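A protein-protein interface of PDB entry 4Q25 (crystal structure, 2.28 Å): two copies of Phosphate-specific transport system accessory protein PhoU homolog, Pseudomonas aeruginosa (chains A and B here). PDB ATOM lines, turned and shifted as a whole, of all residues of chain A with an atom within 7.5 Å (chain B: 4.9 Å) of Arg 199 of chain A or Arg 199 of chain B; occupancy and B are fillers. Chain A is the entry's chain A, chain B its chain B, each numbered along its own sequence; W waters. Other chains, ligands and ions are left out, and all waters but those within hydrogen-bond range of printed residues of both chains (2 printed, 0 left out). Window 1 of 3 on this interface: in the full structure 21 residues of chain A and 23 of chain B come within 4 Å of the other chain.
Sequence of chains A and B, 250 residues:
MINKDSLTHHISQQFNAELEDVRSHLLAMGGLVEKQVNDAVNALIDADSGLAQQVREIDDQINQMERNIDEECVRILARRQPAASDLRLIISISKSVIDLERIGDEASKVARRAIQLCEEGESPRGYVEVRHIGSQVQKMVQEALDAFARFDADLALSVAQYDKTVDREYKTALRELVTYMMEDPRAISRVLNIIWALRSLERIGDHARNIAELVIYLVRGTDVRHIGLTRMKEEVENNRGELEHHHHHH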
ATOM      1  N   GLU A 106     -10.215  33.210 -19.605  1.00  0.00           N
ATOM      2  CA  GLU A 106      -9.861  33.206 -21.009  1.00  0.00           C
ATOM      3  C   GLU A 106      -9.966  34.621 -21.599  1.00  0.00           C
ATOM      4  O   GLU A 106      -9.159  34.990 -22.410  1.00  0.00           O
ATOM      5  CB  GLU A 106     -10.745  32.242 -21.809  1.00  0.00           C
ATOM      6  CG  GLU A 106     -10.577  30.770 -21.457  1.00  0.00           C
ATOM      7  CD  GLU A 106      -9.192  30.219 -21.758  1.00  0.00           C
ATOM      8  OE1 GLU A 106      -8.855  29.154 -21.188  1.00  0.00           O
ATOM      9  OE2 GLU A 106      -8.430  30.823 -22.552  1.00  0.00           O
ATOM     10  N   LYS A 109      -6.850  36.334 -20.760  1.00  0.00           N
ATOM     11  CA  LYS A 109      -5.778  35.955 -21.689  1.00  0.00           C
ATOM     12  C   LYS A 109      -5.862  36.664 -23.055  1.00  0.00           C
ATOM     13  O   LYS A 109      -4.828  37.040 -23.612  1.00  0.00           O
ATOM     14  CB  LYS A 109      -5.722  34.458 -21.923  1.00  0.00           C
ATOM     15  CG  LYS A 109      -5.435  33.643 -20.671  1.00  0.00           C
ATOM     16  CD  LYS A 109      -5.370  32.160 -21.025  1.00  0.00           C
ATOM     17  CE  LYS A 109      -5.681  31.269 -19.834  1.00  0.00           C
ATOM     18  NZ  LYS A 109      -4.882  31.668 -18.659  1.00  0.00           N
ATOM     19  N   VAL A 110      -7.083  36.836 -23.579  1.00  0.00           N
ATOM     20  CA  VAL A 110      -7.303  37.575 -24.838  1.00  0.00           C
ATOM     21  C   VAL A 110      -6.796  38.995 -24.648  1.00  0.00           C
ATOM     22  O   VAL A 110      -6.051  39.491 -25.473  1.00  0.00           O
ATOM     23  CB  VAL A 110      -8.786  37.563 -25.284  1.00  0.00           C
ATOM     24  CG1 VAL A 110      -9.042  38.471 -26.485  1.00  0.00           C
ATOM     25  CG2 VAL A 110      -9.171  36.147 -25.647  1.00  0.00           C
ATOM     26  N   ARG A 113      -3.141  39.101 -24.987  1.00  0.00           N
ATOM     27  CA  ARG A 113      -2.745  39.060 -26.387  1.00  0.00           C
ATOM     28  C   ARG A 113      -2.932  40.422 -26.990  1.00  0.00           C
ATOM     29  O   ARG A 113      -2.142  40.826 -27.767  1.00  0.00           O
ATOM     30  CB  ARG A 113      -3.588  38.064 -27.202  1.00  0.00           C
ATOM     31  CG  ARG A 113      -3.552  36.638 -26.731  1.00  0.00           C
ATOM     32  CD  ARG A 113      -2.149  36.246 -26.385  1.00  0.00           C
ATOM     33  NE  ARG A 113      -2.179  35.135 -25.461  1.00  0.00           N
ATOM     34  CZ  ARG A 113      -1.213  34.864 -24.590  1.00  0.00           C
ATOM     35  NH1 ARG A 113      -1.341  33.809 -23.796  1.00  0.00           N
ATOM     36  NH2 ARG A 113      -0.119  35.641 -24.528  1.00  0.00           N
ATOM     37  N   ILE A 133     -15.442  34.961 -34.590  1.00  0.00           N
ATOM     38  CA  ILE A 133     -15.544  33.918 -33.569  1.00  0.00           C
ATOM     39  C   ILE A 133     -15.892  34.526 -32.207  1.00  0.00           C
ATOM     40  O   ILE A 133     -16.737  34.018 -31.464  1.00  0.00           O
ATOM     41  CB  ILE A 133     -14.249  33.092 -33.547  1.00  0.00           C
ATOM     42  CG1 ILE A 133     -14.152  32.308 -34.847  1.00  0.00           C
ATOM     43  CG2 ILE A 133     -14.202  32.176 -32.344  1.00  0.00           C
ATOM     44  CD1 ILE A 133     -12.942  31.433 -34.992  1.00  0.00           C
ATOM     45  N   ASP A 167     -16.021  25.482 -33.206  1.00  0.00           N
ATOM     46  CA  ASP A 167     -14.774  24.703 -33.238  1.00  0.00           C
ATOM     47  C   ASP A 167     -14.322  24.481 -34.687  1.00  0.00           C
ATOM     48  O   ASP A 167     -13.127  24.435 -34.976  1.00  0.00           O
ATOM     49  CB  ASP A 167     -14.914  23.365 -32.497  1.00  0.00           C
ATOM     50  CG  ASP A 167     -15.306  23.533 -31.010  1.00  0.00           C
ATOM     51  OD1 ASP A 167     -15.090  24.616 -30.418  1.00  0.00           O
ATOM     52  OD2 ASP A 167     -15.852  22.576 -30.407  1.00  0.00           O
ATOM     53  N   TYR A 170     -12.710  27.644 -35.911  1.00  0.00           N
ATOM     54  CA  TYR A 170     -11.411  27.743 -35.305  1.00  0.00           C
ATOM     55  C   TYR A 170     -10.374  26.931 -36.108  1.00  0.00           C
ATOM     56  O   TYR A 170      -9.292  27.433 -36.412  1.00  0.00           O
ATOM     57  CB  TYR A 170     -11.434  27.304 -33.833  1.00  0.00           C
ATOM     58  CG  TYR A 170     -10.040  27.111 -33.277  1.00  0.00           C
ATOM     59  CD1 TYR A 170      -9.273  28.200 -32.893  1.00  0.00           C
ATOM     60  CD2 TYR A 170      -9.461  25.841 -33.201  1.00  0.00           C
ATOM     61  CE1 TYR A 170      -7.973  28.041 -32.436  1.00  0.00           C
ATOM     62  CE2 TYR A 170      -8.174  25.660 -32.730  1.00  0.00           C
ATOM     63  CZ  TYR A 170      -7.430  26.767 -32.346  1.00  0.00           C
ATOM     64  OH  TYR A 170      -6.151  26.613 -31.880  1.00  0.00           O
ATOM     65  N   LYS A 171     -10.700  25.693 -36.464  1.00  0.00           N
ATOM     66  CA  LYS A 171      -9.738  24.838 -37.170  1.00  0.00           C
ATOM     67  C   LYS A 171      -9.404  25.377 -38.562  1.00  0.00           C
ATOM     68  O   LYS A 171      -8.266  25.241 -38.998  1.00  0.00           O
ATOM     69  CB  LYS A 171     -10.221  23.388 -37.241  1.00  0.00           C
ATOM     70  CG  LYS A 171     -10.260  22.703 -35.882  1.00  0.00           C
ATOM     71  CD  LYS A 171     -10.692  21.242 -35.968  1.00  0.00           C
ATOM     72  CE  LYS A 171     -10.361  20.515 -34.673  1.00  0.00           C
ATOM     73  NZ  LYS A 171     -10.683  19.056 -34.720  1.00  0.00           N
ATOM     74  N   LEU A 192       0.993  33.943 -33.797  1.00  0.00           N
ATOM     75  CA  LEU A 192       0.773  33.117 -32.637  1.00  0.00           C
ATOM     76  C   LEU A 192      -0.111  33.800 -31.644  1.00  0.00           C
ATOM     77  O   LEU A 192      -0.931  33.148 -31.022  1.00  0.00           O
ATOM     78  CB  LEU A 192       2.078  32.684 -31.970  1.00  0.00           C
ATOM     79  CG  LEU A 192       2.837  31.638 -32.767  1.00  0.00           C
ATOM     80  CD1 LEU A 192       4.195  31.394 -32.126  1.00  0.00           C
ATOM     81  CD2 LEU A 192       2.050  30.344 -32.845  1.00  0.00           C
ATOM     82  N   ASN A 193       0.059  35.099 -31.465  1.00  0.00           N
ATOM     83  CA  ASN A 193      -0.826  35.838 -30.572  1.00  0.00           C
ATOM     84  C   ASN A 193      -2.304  35.792 -30.992  1.00  0.00           C
ATOM     85  O   ASN A 193      -3.164  35.521 -30.144  1.00  0.00           O
ATOM     86  CB  ASN A 193      -0.300  37.276 -30.327  1.00  0.00           C
ATOM     87  CG  ASN A 193       0.735  37.335 -29.190  1.00  0.00           C
ATOM     88  OD1 ASN A 193       0.403  37.133 -28.021  1.00  0.00           O
ATOM     89  ND2 ASN A 193       1.983  37.616 -29.529  1.00  0.00           N
ATOM     90  N   ILE A 194      -2.605  36.008 -32.283  1.00  0.00           N
ATOM     91  CA  ILE A 194      -3.966  35.811 -32.784  1.00  0.00           C
ATOM     92  C   ILE A 194      -4.457  34.380 -32.543  1.00  0.00           C
ATOM     93  O   ILE A 194      -5.589  34.152 -32.118  1.00  0.00           O
ATOM     94  CB  ILE A 194      -4.117  36.177 -34.266  1.00  0.00           C
ATOM     95  CG1 ILE A 194      -4.819  37.525 -34.442  1.00  0.00           C
ATOM     96  CG2 ILE A 194      -5.181  35.319 -34.906  1.00  0.00           C
ATOM     97  CD1 ILE A 194      -4.001  38.687 -34.125  1.00  0.00           C
ATOM     98  N   ILE A 195      -3.587  33.410 -32.784  1.00  0.00           N
ATOM     99  CA  ILE A 195      -3.916  32.004 -32.576  1.00  0.00           C
ATOM    100  C   ILE A 195      -4.233  31.681 -31.112  1.00  0.00           C
ATOM    101  O   ILE A 195      -5.240  31.030 -30.841  1.00  0.00           O
ATOM    102  CB  ILE A 195      -2.795  31.093 -33.094  1.00  0.00           C
ATOM    103  CG1 ILE A 195      -2.829  31.093 -34.601  1.00  0.00           C
ATOM    104  CG2 ILE A 195      -2.927  29.687 -32.564  1.00  0.00           C
ATOM    105  CD1 ILE A 195      -1.697  30.337 -35.217  1.00  0.00           C
ATOM    106  N   TRP A 196      -3.424  32.175 -30.182  1.00  0.00           N
ATOM    107  CA  TRP A 196      -3.721  31.988 -28.778  1.00  0.00           C
ATOM    108  C   TRP A 196      -5.052  32.654 -28.427  1.00  0.00           C
ATOM    109  O   TRP A 196      -5.838  32.113 -27.667  1.00  0.00           O
ATOM    110  CB  TRP A 196      -2.656  32.553 -27.858  1.00  0.00           C
ATOM    111  CG  TRP A 196      -1.191  32.128 -28.048  1.00  0.00           C
ATOM    112  CD1 TRP A 196      -0.081  32.877 -27.721  1.00  0.00           C
ATOM    113  CD2 TRP A 196      -0.694  30.908 -28.579  1.00  0.00           C
ATOM    114  NE1 TRP A 196       1.053  32.184 -28.002  1.00  0.00           N
ATOM    115  CE2 TRP A 196       0.703  30.972 -28.531  1.00  0.00           C
ATOM    116  CE3 TRP A 196      -1.296  29.759 -29.085  1.00  0.00           C
ATOM    117  CZ2 TRP A 196       1.504  29.946 -28.972  1.00  0.00           C
ATOM    118  CZ3 TRP A 196      -0.502  28.733 -29.533  1.00  0.00           C
ATOM    119  CH2 TRP A 196       0.883  28.830 -29.477  1.00  0.00           C
ATOM    120  N   ALA A 197      -5.273  33.859 -28.915  1.00  0.00           N
ATOM    121  CA  ALA A 197      -6.546  34.538 -28.657  1.00  0.00           C
ATOM    122  C   ALA A 197      -7.749  33.719 -29.206  1.00  0.00           C
ATOM    123  O   ALA A 197      -8.731  33.491 -28.515  1.00  0.00           O
ATOM    124  CB  ALA A 197      -6.521  35.927 -29.245  1.00  0.00           C
ATOM    125  N   LEU A 198      -7.653  33.263 -30.440  1.00  0.00           N
ATOM    126  CA  LEU A 198      -8.679  32.373 -31.030  1.00  0.00           C
ATOM    127  C   LEU A 198      -8.922  31.100 -30.216  1.00  0.00           C
ATOM    128  O   LEU A 198     -10.062  30.689 -30.063  1.00  0.00           O
ATOM    129  CB  LEU A 198      -8.315  31.969 -32.466  1.00  0.00           C
ATOM    130  CG  LEU A 198      -8.427  33.087 -33.496  1.00  0.00           C
ATOM    131  CD1 LEU A 198      -7.758  32.691 -34.778  1.00  0.00           C
ATOM    132  CD2 LEU A 198      -9.864  33.436 -33.789  1.00  0.00           C
ATOM    133  N   ARG A 199      -7.869  30.497 -29.680  1.00  0.00           N
ATOM    134  CA  ARG A 199      -7.997  29.307 -28.849  1.00  0.00           C
ATOM    135  C   ARG A 199      -8.756  29.615 -27.558  1.00  0.00           C
ATOM    136  O   ARG A 199      -9.641  28.849 -27.154  1.00  0.00           O
ATOM    137  CB  ARG A 199      -6.615  28.711 -28.571  1.00  0.00           C
ATOM    138  CG  ARG A 199      -6.589  27.562 -27.576  1.00  0.00           C
ATOM    139  CD  ARG A 199      -7.145  26.298 -28.199  1.00  0.00           C
ATOM    140  NE  ARG A 199      -7.647  25.359 -27.196  1.00  0.00           N
ATOM    141  CZ  ARG A 199      -8.266  24.216 -27.490  1.00  0.00           C
ATOM    142  NH1 ARG A 199      -8.478  23.862 -28.757  1.00  0.00           N
ATOM    143  NH2 ARG A 199      -8.670  23.421 -26.523  1.00  0.00           N
ATOM    144  N   SER A 200      -8.434  30.729 -26.915  1.00  0.00           N
ATOM    145  CA  SER A 200      -9.236  31.234 -25.801  1.00  0.00           C
ATOM    146  C   SER A 200     -10.712  31.533 -26.177  1.00  0.00           C
ATOM    147  O   SER A 200     -11.625  31.288 -25.405  1.00  0.00           O
ATOM    148  CB  SER A 200      -8.595  32.510 -25.212  1.00  0.00           C
ATOM    149  OG  SER A 200      -7.325  32.254 -24.591  1.00  0.00           O
ATOM    150  N   LEU A 201     -10.957  32.111 -27.342  1.00  0.00           N
ATOM    151  CA  LEU A 201     -12.359  32.328 -27.738  1.00  0.00           C
ATOM    152  C   LEU A 201     -13.108  30.969 -27.938  1.00  0.00           C
ATOM    153  O   LEU A 201     -14.249  30.813 -27.551  1.00  0.00           O
ATOM    154  CB  LEU A 201     -12.425  33.217 -28.985  1.00  0.00           C
ATOM    155  CG  LEU A 201     -11.982  34.666 -28.758  1.00  0.00           C
ATOM    156  CD1 LEU A 201     -11.961  35.447 -30.065  1.00  0.00           C
ATOM    157  CD2 LEU A 201     -12.876  35.362 -27.750  1.00  0.00           C
ATOM    158  N   GLU A 202     -12.438  29.991 -28.510  1.00  0.00           N
ATOM    159  CA  GLU A 202     -13.007  28.675 -28.687  1.00  0.00           C
ATOM    160  C   GLU A 202     -13.353  28.041 -27.344  1.00  0.00           C
ATOM    161  O   GLU A 202     -14.396  27.418 -27.204  1.00  0.00           O
ATOM    162  CB  GLU A 202     -12.047  27.764 -29.440  1.00  0.00           C
ATOM    163  CG  GLU A 202     -12.654  26.412 -29.713  1.00  0.00           C
ATOM    164  CD  GLU A 202     -11.729  25.433 -30.401  1.00  0.00           C
ATOM    165  OE1 GLU A 202     -12.249  24.521 -31.072  1.00  0.00           O
ATOM    166  OE2 GLU A 202     -10.499  25.551 -30.258  1.00  0.00           O
ATOM    167  N   ARG A 203     -12.470  28.202 -26.364  1.00  0.00           N
ATOM    168  CA  ARG A 203     -12.726  27.698 -25.039  1.00  0.00           C
ATOM    169  C   ARG A 203     -13.887  28.425 -24.388  1.00  0.00           C
ATOM    170  O   ARG A 203     -14.692  27.837 -23.685  1.00  0.00           O
ATOM    171  CB  ARG A 203     -11.496  27.847 -24.174  1.00  0.00           C
ATOM    172  CG  ARG A 203     -10.333  26.929 -24.532  1.00  0.00           C
ATOM    173  CD  ARG A 203     -10.233  25.798 -23.544  1.00  0.00           C
ATOM    174  NE  ARG A 203     -11.271  24.785 -23.725  1.00  0.00           N
ATOM    175  CZ  ARG A 203     -11.778  24.019 -22.754  1.00  0.00           C
ATOM    176  NH1 ARG A 203     -11.394  24.146 -21.467  1.00  0.00           N
ATOM    177  NH2 ARG A 203     -12.716  23.134 -23.075  1.00  0.00           N
ATOM    178  N   ILE A 204     -13.979  29.722 -24.599  1.00  0.00           N
ATOM    179  CA  ILE A 204     -15.140  30.437 -24.089  1.00  0.00           C
ATOM    180  C   ILE A 204     -16.462  29.817 -24.627  1.00  0.00           C
ATOM    181  O   ILE A 204     -17.419  29.664 -23.892  1.00  0.00           O
ATOM    182  CB  ILE A 204     -15.017  31.917 -24.385  1.00  0.00           C
ATOM    183  CG1 ILE A 204     -13.913  32.496 -23.497  1.00  0.00           C
ATOM    184  CG2 ILE A 204     -16.333  32.649 -24.137  1.00  0.00           C
ATOM    185  CD1 ILE A 204     -13.530  33.911 -23.851  1.00  0.00           C
ATOM    186  N   GLY A 205     -16.467  29.431 -25.891  1.00  0.00           N
ATOM    187  CA  GLY A 205     -17.604  28.765 -26.483  1.00  0.00           C
ATOM    188  C   GLY A 205     -17.811  27.366 -25.946  1.00  0.00           C
ATOM    189  O   GLY A 205     -18.944  26.955 -25.765  1.00  0.00           O
ATOM    190  N   ASP A 206     -16.727  26.623 -25.719  1.00  0.00           N
ATOM    191  CA  ASP A 206     -16.837  25.322 -25.046  1.00  0.00           C
ATOM    192  C   ASP A 206     -17.505  25.470 -23.678  1.00  0.00           C
ATOM    193  O   ASP A 206     -18.371  24.683 -23.355  1.00  0.00           O
ATOM    194  CB  ASP A 206     -15.481  24.652 -24.891  1.00  0.00           C
ATOM    195  CG  ASP A 206     -14.868  24.267 -26.200  1.00  0.00           C
ATOM    196  OD1 ASP A 206     -15.521  24.409 -27.269  1.00  0.00           O
ATOM    197  OD2 ASP A 206     -13.692  23.861 -26.149  1.00  0.00           O
ATOM    198  N   LYS B 109      -3.387  15.453 -25.393  1.00  0.00           N
ATOM    199  CA  LYS B 109      -2.901  16.388 -26.393  1.00  0.00           C
ATOM    200  C   LYS B 109      -1.406  16.306 -26.550  1.00  0.00           C
ATOM    201  O   LYS B 109      -0.895  16.422 -27.657  1.00  0.00           O
ATOM    202  CB  LYS B 109      -3.287  17.832 -26.082  1.00  0.00           C
ATOM    203  CG  LYS B 109      -4.775  18.117 -26.255  1.00  0.00           C
ATOM    204  CD  LYS B 109      -5.066  19.582 -25.981  1.00  0.00           C
ATOM    205  CE  LYS B 109      -6.476  19.787 -25.467  1.00  0.00           C
ATOM    206  NZ  LYS B 109      -7.460  19.400 -26.504  1.00  0.00           N
ATOM    207  N   TYR B 170       7.876  28.628 -18.893  1.00  0.00           N
ATOM    208  CA  TYR B 170       7.145  28.564 -20.161  1.00  0.00           C
ATOM    209  C   TYR B 170       7.338  29.845 -21.022  1.00  0.00           C
ATOM    210  O   TYR B 170       7.651  29.770 -22.175  1.00  0.00           O
ATOM    211  CB  TYR B 170       5.634  28.267 -19.961  1.00  0.00           C
ATOM    212  CG  TYR B 170       4.886  28.384 -21.267  1.00  0.00           C
ATOM    213  CD1 TYR B 170       4.973  27.383 -22.239  1.00  0.00           C
ATOM    214  CD2 TYR B 170       4.172  29.526 -21.565  1.00  0.00           C
ATOM    215  CE1 TYR B 170       4.341  27.504 -23.470  1.00  0.00           C
ATOM    216  CE2 TYR B 170       3.528  29.670 -22.793  1.00  0.00           C
ATOM    217  CZ  TYR B 170       3.622  28.654 -23.744  1.00  0.00           C
ATOM    218  OH  TYR B 170       2.998  28.813 -24.953  1.00  0.00           O
ATOM    219  N   ILE B 195       5.762  23.633 -28.996  1.00  0.00           N
ATOM    220  CA  ILE B 195       5.034  24.727 -28.352  1.00  0.00           C
ATOM    221  C   ILE B 195       3.618  24.302 -27.878  1.00  0.00           C
ATOM    222  O   ILE B 195       3.183  24.664 -26.761  1.00  0.00           O
ATOM    223  CB  ILE B 195       4.974  25.940 -29.273  1.00  0.00           C
ATOM    224  CG1 ILE B 195       6.375  26.490 -29.485  1.00  0.00           C
ATOM    225  CG2 ILE B 195       4.076  27.026 -28.694  1.00  0.00           C
ATOM    226  CD1 ILE B 195       6.468  27.700 -30.400  1.00  0.00           C
ATOM    227  N   TRP B 196       2.898  23.561 -28.720  1.00  0.00           N
ATOM    228  CA  TRP B 196       1.547  23.116 -28.342  1.00  0.00           C
ATOM    229  C   TRP B 196       1.629  22.204 -27.126  1.00  0.00           C
ATOM    230  O   TRP B 196       0.829  22.349 -26.194  1.00  0.00           O
ATOM    231  CB  TRP B 196       0.821  22.416 -29.485  1.00  0.00           C
ATOM    232  CG  TRP B 196       0.161  23.321 -30.428  1.00  0.00           C
ATOM    233  CD1 TRP B 196       0.549  23.600 -31.698  1.00  0.00           C
ATOM    234  CD2 TRP B 196      -1.056  24.039 -30.214  1.00  0.00           C
ATOM    235  NE1 TRP B 196      -0.323  24.470 -32.277  1.00  0.00           N
ATOM    236  CE2 TRP B 196      -1.320  24.765 -31.388  1.00  0.00           C
ATOM    237  CE3 TRP B 196      -1.940  24.160 -29.129  1.00  0.00           C
ATOM    238  CZ2 TRP B 196      -2.433  25.606 -31.519  1.00  0.00           C
ATOM    239  CZ3 TRP B 196      -3.060  25.019 -29.248  1.00  0.00           C
ATOM    240  CH2 TRP B 196      -3.297  25.716 -30.443  1.00  0.00           C
ATOM    241  N   ALA B 197       2.593  21.276 -27.136  1.00  0.00           N
ATOM    242  CA  ALA B 197       2.818  20.385 -26.011  1.00  0.00           C
ATOM    243  C   ALA B 197       3.122  21.167 -24.746  1.00  0.00           C
ATOM    244  O   ALA B 197       2.571  20.860 -23.695  1.00  0.00           O
ATOM    245  CB  ALA B 197       3.941  19.414 -26.316  1.00  0.00           C
ATOM    246  N   LEU B 198       3.992  22.184 -24.853  1.00  0.00           N
ATOM    247  CA  LEU B 198       4.326  23.040 -23.725  1.00  0.00           C
ATOM    248  C   LEU B 198       3.131  23.779 -23.184  1.00  0.00           C
ATOM    249  O   LEU B 198       2.990  23.924 -21.967  1.00  0.00           O
ATOM    250  CB  LEU B 198       5.402  24.045 -24.107  1.00  0.00           C
ATOM    251  CG  LEU B 198       6.786  23.467 -24.372  1.00  0.00           C
ATOM    252  CD1 LEU B 198       7.725  24.527 -24.909  1.00  0.00           C
ATOM    253  CD2 LEU B 198       7.315  22.842 -23.098  1.00  0.00           C
ATOM    254  N   ARG B 199       2.281  24.272 -24.085  1.00  0.00           N
ATOM    255  CA  ARG B 199       0.994  24.851 -23.683  1.00  0.00           C
ATOM    256  C   ARG B 199       0.144  23.888 -22.832  1.00  0.00           C
ATOM    257  O   ARG B 199      -0.405  24.275 -21.815  1.00  0.00           O
ATOM    258  CB  ARG B 199       0.211  25.355 -24.898  1.00  0.00           C
ATOM    259  CG  ARG B 199       0.693  26.728 -25.375  1.00  0.00           C
ATOM    260  CD  ARG B 199      -0.019  27.228 -26.648  1.00  0.00           C
ATOM    261  NE  ARG B 199      -1.481  27.310 -26.511  1.00  0.00           N
ATOM    262  CZ  ARG B 199      -2.161  28.365 -26.042  1.00  0.00           C
ATOM    263  NH1 ARG B 199      -1.525  29.455 -25.645  1.00  0.00           N
ATOM    264  NH2 ARG B 199      -3.500  28.333 -25.972  1.00  0.00           N
ATOM    265  N   SER B 200       0.078  22.637 -23.219  1.00  0.00           N
ATOM    266  CA  SER B 200      -0.668  21.649 -22.447  1.00  0.00           C
ATOM    267  C   SER B 200      -0.075  21.410 -21.089  1.00  0.00           C
ATOM    268  O   SER B 200      -0.814  21.352 -20.109  1.00  0.00           O
ATOM    269  CB  SER B 200      -0.770  20.332 -23.199  1.00  0.00           C
ATOM    270  OG  SER B 200      -1.773  20.469 -24.166  1.00  0.00           O
ATOM    271  N   LEU B 201       1.254  21.321 -21.023  1.00  0.00           N
ATOM    272  CA  LEU B 201       1.962  21.112 -19.744  1.00  0.00           C
ATOM    273  C   LEU B 201       1.730  22.277 -18.753  1.00  0.00           C
ATOM    274  O   LEU B 201       1.464  22.069 -17.564  1.00  0.00           O
ATOM    275  CB  LEU B 201       3.461  20.900 -19.986  1.00  0.00           C
ATOM    276  CG  LEU B 201       3.831  19.654 -20.774  1.00  0.00           C
ATOM    277  CD1 LEU B 201       5.317  19.663 -21.064  1.00  0.00           C
ATOM    278  CD2 LEU B 201       3.422  18.407 -20.015  1.00  0.00           C
ATOM    279  N   GLU B 202       1.814  23.486 -19.260  1.00  0.00           N
ATOM    280  CA  GLU B 202       1.549  24.668 -18.460  1.00  0.00           C
ATOM    281  C   GLU B 202       0.114  24.587 -17.912  1.00  0.00           C
ATOM    282  O   GLU B 202      -0.146  24.960 -16.759  1.00  0.00           O
ATOM    283  CB  GLU B 202       1.761  25.953 -19.290  1.00  0.00           C
ATOM    284  CG  GLU B 202       1.324  27.234 -18.586  1.00  0.00           C
ATOM    285  CD  GLU B 202       1.485  28.503 -19.441  1.00  0.00           C
ATOM    286  OE1 GLU B 202       1.746  29.584 -18.850  1.00  0.00           O
ATOM    287  OE2 GLU B 202       1.357  28.433 -20.691  1.00  0.00           O
ATOM    288  N   ARG B 203      -0.799  24.144 -18.746  1.00  0.00           N
ATOM    289  CA  ARG B 203      -2.159  23.932 -18.342  1.00  0.00           C
ATOM    290  C   ARG B 203      -2.338  22.850 -17.289  1.00  0.00           C
ATOM    291  O   ARG B 203      -3.149  22.978 -16.440  1.00  0.00           O
ATOM    292  CB  ARG B 203      -3.067  23.729 -19.550  1.00  0.00           C
ATOM    293  CG  ARG B 203      -3.803  24.981 -19.968  1.00  0.00           C
ATOM    294  CD  ARG B 203      -3.824  25.250 -21.458  1.00  0.00           C
ATOM    295  NE  ARG B 203      -4.109  24.067 -22.268  1.00  0.00           N
ATOM    296  CZ  ARG B 203      -4.053  24.008 -23.600  1.00  0.00           C
ATOM    297  NH1 ARG B 203      -3.740  25.073 -24.307  1.00  0.00           N
ATOM    298  NH2 ARG B 203      -4.341  22.891 -24.220  1.00  0.00           N
HETATM  299  O   HOH W   1      -4.983  30.655 -25.725  1.00  0.00           O
HETATM  300  O   HOH W   2      -6.997  26.085 -24.401  1.00  0.00           O
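Tyr 170 of chain A touches Trp 196 of chain B, but with the chains exchanged Trp 196 of chain A does not touch Tyr 170 of chain B (4.4 Å).
Trp 196 of chain A touches Ile 195 of chain B, but with the chains exchanged Ile 195 of chain A does not touch Trp 196 of chain B (4.2 Å).
Trp 196 of chain A touches Arg 199 of chain B, but with the chains exchanged Arg 199 of chain A does not touch Trp 196 of chain B (4.4 Å).
Arg 199 of chain B touches its own counterpart, Arg 199 of chain A.
Positions printed for both chains: 109, 170, 195, 196, 197, 198, 199, 200, 201, 202 and 203.
Of the printed residues of chain B, Tyr 170 of chain A touches Trp 196 (3.3 Å).
Of the printed residues of chain A, Ile 195 of chain B touches Trp 196.
Of the printed residues of chain A, Trp 196 of chain B touches Tyr 170.
Arg 199 of chain B touches two residues of chain A.
The backbone carbonyl oxygen (O) of Trp 196 of chain A lies within hydrogen-bond range of the side-chain hydroxyl (OG) of Ser 200 of chain A, at 3.4 Å.
The side-chain carboxylate (OE2) of Glu 202 of chain A lies within salt-bridge range of the guanidinium group (NH1) of Arg 199 of chain A, at 3.0 Å.
Of the 23 printed residues of chain A, 3 touch a printed residue of chain B.
Hydrophobic or aromatic side chains of chain A within 4 Å of the printed part of chain B: Tyr 170 and Trp 196.
Hydrophobic or aromatic side chains of chain B within 4 Å of the printed part of chain A: Ile 195 and Trp 196.
Among the printed residues, 4 pairs touch across the chains.
Among the printed residues, no Asp or Glu carboxylate lies within 4 Å of a Lys or Arg side-chain nitrogen of the other chain.
Trp 196 of chain B touches Tyr 170 of chain A (CH2 to OH, 3.3 Å).
Trp 196 of chain A touches Ile 195 of chain B.
CD of Arg 199 of chain B touches CZ3 of Trp 196 of chain A, 3.3 Å away.
Arg 199 of chain A touches Arg 199 of chain B.
Water W1 lies within hydrogen-bond range of the backbone carbonyl oxygen (O) of Trp 196 of chain A (2.6 Å), the guanidinium group (NH2) of Arg 199 of chain B (2.8 Å) and the side-chain hydroxyl (OG) of Ser 200 of chain A (3.1 Å).
Water W2 lies within hydrogen-bond range of the guanidinium group of Arg 199 of chain A (3.0 Å) and the guanidinium group of Arg 203 of chain B (3.4 Å).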
